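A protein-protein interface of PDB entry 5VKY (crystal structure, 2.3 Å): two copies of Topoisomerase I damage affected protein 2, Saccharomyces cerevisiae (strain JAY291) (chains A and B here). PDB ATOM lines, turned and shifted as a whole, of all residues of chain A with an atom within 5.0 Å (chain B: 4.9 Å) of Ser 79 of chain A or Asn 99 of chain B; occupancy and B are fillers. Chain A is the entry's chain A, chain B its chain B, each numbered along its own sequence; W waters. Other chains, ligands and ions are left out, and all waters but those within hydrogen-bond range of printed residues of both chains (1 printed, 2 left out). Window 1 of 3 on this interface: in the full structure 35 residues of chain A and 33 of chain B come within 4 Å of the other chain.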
ATOM      1  N   ILE A  60      22.837  -2.149 -25.700  1.00  0.00           N
ATOM      2  CA  ILE A  60      22.233  -0.825 -25.778  1.00  0.00           C
ATOM      3  C   ILE A  60      23.295   0.262 -25.734  1.00  0.00           C
ATOM      4  O   ILE A  60      23.219   1.258 -26.467  1.00  0.00           O
ATOM      5  CB  ILE A  60      21.208  -0.654 -24.649  1.00  0.00           C
ATOM      6  CG1 ILE A  60      19.961  -1.464 -24.985  1.00  0.00           C
ATOM      7  CG2 ILE A  60      20.915   0.837 -24.410  1.00  0.00           C
ATOM      8  CD1 ILE A  60      19.058  -1.729 -23.776  1.00  0.00           C
ATOM      9  N   ILE A  77      17.110   6.558 -28.834  1.00  0.00           N
ATOM     10  CA  ILE A  77      16.632   5.639 -27.809  1.00  0.00           C
ATOM     11  C   ILE A  77      16.850   4.228 -28.328  1.00  0.00           C
ATOM     12  O   ILE A  77      16.567   3.939 -29.500  1.00  0.00           O
ATOM     13  CB  ILE A  77      15.146   5.885 -27.483  1.00  0.00           C
ATOM     14  CG1 ILE A  77      14.993   7.151 -26.635  1.00  0.00           C
ATOM     15  CG2 ILE A  77      14.562   4.703 -26.749  1.00  0.00           C
ATOM     16  CD1 ILE A  77      13.771   7.938 -26.981  1.00  0.00           C
ATOM     17  N   ALA A  78      17.385   3.356 -27.486  1.00  0.00           N
ATOM     18  CA  ALA A  78      17.547   1.959 -27.872  1.00  0.00           C
ATOM     19  C   ALA A  78      16.849   1.092 -26.837  1.00  0.00           C
ATOM     20  O   ALA A  78      17.142   1.186 -25.641  1.00  0.00           O
ATOM     21  CB  ALA A  78      19.022   1.567 -28.021  1.00  0.00           C
ATOM     22  N   SER A  79      15.934   0.257 -27.302  1.00  0.00           N
ATOM     23  CA  SER A  79      15.119  -0.598 -26.461  1.00  0.00           C
ATOM     24  C   SER A  79      15.337  -2.047 -26.870  1.00  0.00           C
ATOM     25  O   SER A  79      15.215  -2.380 -28.048  1.00  0.00           O
ATOM     26  CB  SER A  79      13.646  -0.199 -26.601  1.00  0.00           C
ATOM     27  OG  SER A  79      12.824  -1.125 -25.947  1.00  0.00           O
ATOM     28  N   VAL A  80      15.651  -2.910 -25.904  1.00  0.00           N
ATOM     29  CA  VAL A  80      15.867  -4.328 -26.183  1.00  0.00           C
ATOM     30  C   VAL A  80      14.932  -5.144 -25.312  1.00  0.00           C
ATOM     31  O   VAL A  80      14.956  -5.010 -24.082  1.00  0.00           O
ATOM     32  CB  VAL A  80      17.321  -4.764 -25.942  1.00  0.00           C
ATOM     33  CG1 VAL A  80      17.454  -6.263 -26.203  1.00  0.00           C
ATOM     34  CG2 VAL A  80      18.270  -3.962 -26.822  1.00  0.00           C
ATOM     35  N   THR A  81      14.115  -5.990 -25.948  1.00  0.00           N
ATOM     36  CA  THR A  81      13.362  -7.023 -25.249  1.00  0.00           C
ATOM     37  C   THR A  81      14.142  -8.338 -25.282  1.00  0.00           C
ATOM     38  O   THR A  81      14.608  -8.764 -26.348  1.00  0.00           O
ATOM     39  CB  THR A  81      11.972  -7.217 -25.874  1.00  0.00           C
ATOM     40  OG1 THR A  81      11.261  -5.970 -25.867  1.00  0.00           O
ATOM     41  CG2 THR A  81      11.157  -8.214 -25.065  1.00  0.00           C
ATOM     42  N   THR A  82      14.279  -8.975 -24.119  1.00  0.00           N
ATOM     43  CA  THR A  82      14.973 -10.249 -23.970  1.00  0.00           C
ATOM     44  C   THR A  82      13.947 -11.334 -23.673  1.00  0.00           C
ATOM     45  O   THR A  82      13.246 -11.270 -22.653  1.00  0.00           O
ATOM     46  CB  THR A  82      16.026 -10.174 -22.858  1.00  0.00           C
ATOM     47  OG1 THR A  82      16.957  -9.128 -23.150  1.00  0.00           O
ATOM     48  CG2 THR A  82      16.791 -11.473 -22.738  1.00  0.00           C
ATOM     49  N   LEU A 127      14.858  -8.694 -29.290  1.00  0.00           N
ATOM     50  CA  LEU A 127      14.195  -7.830 -30.256  1.00  0.00           C
ATOM     51  C   LEU A 127      14.633  -6.412 -29.933  1.00  0.00           C
ATOM     52  O   LEU A 127      14.288  -5.885 -28.875  1.00  0.00           O
ATOM     53  CB  LEU A 127      12.675  -7.998 -30.171  1.00  0.00           C
ATOM     54  CG  LEU A 127      11.798  -7.304 -31.213  1.00  0.00           C
ATOM     55  CD1 LEU A 127      12.318  -7.552 -32.585  1.00  0.00           C
ATOM     56  CD2 LEU A 127      10.349  -7.825 -31.101  1.00  0.00           C
ATOM     57  N   ILE A 128      15.412  -5.802 -30.814  1.00  0.00           N
ATOM     58  CA  ILE A 128      15.943  -4.465 -30.579  1.00  0.00           C
ATOM     59  C   ILE A 128      15.190  -3.466 -31.446  1.00  0.00           C
ATOM     60  O   ILE A 128      14.933  -3.717 -32.630  1.00  0.00           O
ATOM     61  CB  ILE A 128      17.466  -4.390 -30.824  1.00  0.00           C
ATOM     62  CG1 ILE A 128      17.999  -3.022 -30.391  1.00  0.00           C
ATOM     63  CG2 ILE A 128      17.805  -4.596 -32.294  1.00  0.00           C
ATOM     64  CD1 ILE A 128      19.491  -2.949 -30.298  1.00  0.00           C
ATOM     65  N   THR A 129      14.852  -2.325 -30.852  1.00  0.00           N
ATOM     66  CA  THR A 129      14.208  -1.227 -31.550  1.00  0.00           C
ATOM     67  C   THR A 129      15.045   0.023 -31.357  1.00  0.00           C
ATOM     68  O   THR A 129      15.383   0.380 -30.222  1.00  0.00           O
ATOM     69  CB  THR A 129      12.788  -0.979 -31.034  1.00  0.00           C
ATOM     70  OG1 THR A 129      12.016  -2.187 -31.119  1.00  0.00           O
ATOM     71  CG2 THR A 129      12.124   0.121 -31.853  1.00  0.00           C
ATOM     72  N   LEU B  97      10.052 -12.577 -20.076  1.00  0.00           N
ATOM     73  CA  LEU B  97      10.084 -11.470 -21.014  1.00  0.00           C
ATOM     74  C   LEU B  97      10.540 -10.245 -20.244  1.00  0.00           C
ATOM     75  O   LEU B  97       9.875  -9.853 -19.285  1.00  0.00           O
ATOM     76  CB  LEU B  97       8.696 -11.245 -21.615  1.00  0.00           C
ATOM     77  CG  LEU B  97       8.555 -10.587 -22.975  1.00  0.00           C
ATOM     78  CD1 LEU B  97       9.385 -11.310 -24.039  1.00  0.00           C
ATOM     79  CD2 LEU B  97       7.084 -10.575 -23.366  1.00  0.00           C
ATOM     80  N   LYS B  98      11.660  -9.643 -20.659  1.00  0.00           N
ATOM     81  CA  LYS B  98      12.192  -8.447 -20.018  1.00  0.00           C
ATOM     82  C   LYS B  98      12.413  -7.363 -21.059  1.00  0.00           C
ATOM     83  O   LYS B  98      12.537  -7.643 -22.258  1.00  0.00           O
ATOM     84  CB  LYS B  98      13.524  -8.706 -19.287  1.00  0.00           C
ATOM     85  CG  LYS B  98      13.519  -9.928 -18.385  1.00  0.00           C
ATOM     86  CD  LYS B  98      13.127  -9.546 -16.973  1.00  0.00           C
ATOM     87  CE  LYS B  98      13.171 -10.741 -16.023  1.00  0.00           C
ATOM     88  NZ  LYS B  98      12.011 -10.692 -15.080  1.00  0.00           N
ATOM     89  N   ASN B  99      12.475  -6.115 -20.585  1.00  0.00           N
ATOM     90  CA  ASN B  99      12.830  -5.002 -21.453  1.00  0.00           C
ATOM     91  C   ASN B  99      13.850  -4.081 -20.807  1.00  0.00           C
ATOM     92  O   ASN B  99      13.772  -3.793 -19.611  1.00  0.00           O
ATOM     93  CB  ASN B  99      11.633  -4.145 -21.842  1.00  0.00           C
ATOM     94  CG  ASN B  99      11.967  -3.226 -23.004  1.00  0.00           C
ATOM     95  OD1 ASN B  99      12.101  -3.682 -24.134  1.00  0.00           O
ATOM     96  ND2 ASN B  99      12.161  -1.949 -22.725  1.00  0.00           N
ATOM     97  N   ASP B 100      14.767  -3.568 -21.624  1.00  0.00           N
ATOM     98  CA  ASP B 100      15.689  -2.533 -21.191  1.00  0.00           C
ATOM     99  C   ASP B 100      15.680  -1.406 -22.205  1.00  0.00           C
ATOM    100  O   ASP B 100      15.417  -1.623 -23.382  1.00  0.00           O
ATOM    101  CB  ASP B 100      17.099  -3.074 -21.034  1.00  0.00           C
ATOM    102  CG  ASP B 100      17.148  -4.239 -20.118  1.00  0.00           C
ATOM    103  OD1 ASP B 100      17.024  -4.048 -18.888  1.00  0.00           O
ATOM    104  OD2 ASP B 100      17.267  -5.359 -20.629  1.00  0.00           O
ATOM    105  N   ILE B 101      16.010  -0.207 -21.742  1.00  0.00           N
ATOM    106  CA  ILE B 101      15.913   0.983 -22.570  1.00  0.00           C
ATOM    107  C   ILE B 101      17.021   1.941 -22.169  1.00  0.00           C
ATOM    108  O   ILE B 101      17.251   2.186 -20.983  1.00  0.00           O
ATOM    109  CB  ILE B 101      14.521   1.632 -22.441  1.00  0.00           C
ATOM    110  CG1 ILE B 101      14.397   2.841 -23.363  1.00  0.00           C
ATOM    111  CG2 ILE B 101      14.251   2.043 -21.012  1.00  0.00           C
ATOM    112  CD1 ILE B 101      13.016   2.874 -24.047  1.00  0.00           C
ATOM    113  N   ASN B 114       7.596   0.001 -17.092  1.00  0.00           N
ATOM    114  CA  ASN B 114       7.278  -1.281 -17.704  1.00  0.00           C
ATOM    115  C   ASN B 114       6.099  -1.929 -16.992  1.00  0.00           C
ATOM    116  O   ASN B 114       5.986  -1.874 -15.759  1.00  0.00           O
ATOM    117  CB  ASN B 114       8.450  -2.260 -17.640  1.00  0.00           C
ATOM    118  CG  ASN B 114       9.716  -1.725 -18.293  1.00  0.00           C
ATOM    119  OD1 ASN B 114       9.718  -1.318 -19.461  1.00  0.00           O
ATOM    120  ND2 ASN B 114      10.818  -1.770 -17.545  1.00  0.00           N
ATOM    121  N   LEU B 127       4.281  -6.972 -23.118  1.00  0.00           N
ATOM    122  CA  LEU B 127       5.165  -6.140 -22.315  1.00  0.00           C
ATOM    123  C   LEU B 127       5.085  -4.730 -22.876  1.00  0.00           C
ATOM    124  O   LEU B 127       5.523  -4.483 -24.002  1.00  0.00           O
ATOM    125  CB  LEU B 127       6.601  -6.664 -22.347  1.00  0.00           C
ATOM    126  CG  LEU B 127       7.591  -6.035 -21.355  1.00  0.00           C
ATOM    127  CD1 LEU B 127       7.015  -5.986 -19.975  1.00  0.00           C
ATOM    128  CD2 LEU B 127       8.918  -6.840 -21.359  1.00  0.00           C
ATOM    129  N   THR B 129       5.977  -0.632 -22.418  1.00  0.00           N
ATOM    130  CA  THR B 129       6.916   0.306 -21.829  1.00  0.00           C
ATOM    131  C   THR B 129       6.465   1.715 -22.177  1.00  0.00           C
ATOM    132  O   THR B 129       6.255   2.041 -23.357  1.00  0.00           O
ATOM    133  CB  THR B 129       8.334   0.064 -22.356  1.00  0.00           C
ATOM    134  OG1 THR B 129       8.738  -1.271 -22.044  1.00  0.00           O
ATOM    135  CG2 THR B 129       9.312   1.056 -21.740  1.00  0.00           C
HETATM  136  O   HOH W   1      16.088  -6.986 -22.173  1.00  0.00           O
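The side-chain amide oxygen of Asn 99 of chain B is in hydrogen-bond range of the side-chain hydroxyl of Ser 79 of chain A, at 3.2 Å.
O of Val 80 of chain A sits close to OD1 of Asn 99 of chain B (3.1 Å).
The backbone NH (N) of Val 80 of chain A sits at hydrogen-bond distance from the backbone carbonyl oxygen (O) of Asp 100 of chain B, 2.8 Å away.
The side-chain amide oxygen (OD1) of Asn 99 of chain B lies within hydrogen-bond range of the side-chain hydroxyl (OG1) of Thr 81 of chain A (3.0 Å).
N of Thr 82 of chain A sits at hydrogen-bond distance from O of Lys 98 of chain B (2.9 Å).
Water W1 lies within hydrogen-bond range of the side-chain hydroxyl of Thr 82 of chain A (2.5 Å), the side-chain carboxylate of Asp 100 of chain B (2.5 Å) and the backbone carbonyl oxygen of Val 80 of chain A (3.0 Å).
2 positions are printed for both chains.
Of the 14 pairs that touch across the chains among the printed residues, none has its exchanged pair printed and touching as well.
Among the printed residues, merely in contact across the chains: Thr 81 of chain A with Lys 98 of chain B (3.2 Å), Ser 79 of chain A with Asp 100 of chain B (3.3 Å), Ala 78 of chain A with Ile 101 of chain B (3.3 Å), Thr 82 of chain A with Leu 97 of chain B (3.6 Å), Ile 77 of chain A with Ile 101 of chain B (3.6 Å), Ile 60 of chain A with Asp 100 of chain B (3.6 Å), Thr 81 of chain A with Leu 97 of chain B (3.7 Å), Ile 60 of chain A with Ile 101 of chain B (3.97 Å) and Ala 78 of chain A with Asp 100 of chain B (3.996 Å).
Ser 79 of chain A touches two residues of chain B.
Asn 99 of chain B touches just these residues of chain A: Ser 79 (3.2 Å), Val 80 (3.1 Å) and Thr 81 (3.0 Å).
Of the printed residues of chain B, Ile 60 of chain A touches Asp 100 and Ile 101.
Printed residues of chain B within 4 Å of Val 80 of chain A: Asn 99 (3.1 Å) and Asp 100 (2.8 Å).
The nearest residue of chain A that does not touch Asn 99 of chain B is Thr 82 of chain A (4.9 Å).
Hydrophobic or aromatic side chains of chain A that line the printed part of chain B: Ile 60 and Ile 77.
Of the 8 printed residues of chain B, 5 touch a printed residue of chain A.
Among the printed residues, no Asp or Glu carboxylate lies within 4 Å of a Lys or Arg side-chain nitrogen of the other chain.
The backbone carbonyl oxygen (O) of Ser 79 of chain A lies within hydrogen-bond range of the backbone NH (N) of Thr 129 of chain A, 2.8 Å away.
N of Thr 81 of chain A is in hydrogen-bond range of O of Leu 127 of chain A, at 2.9 Å.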
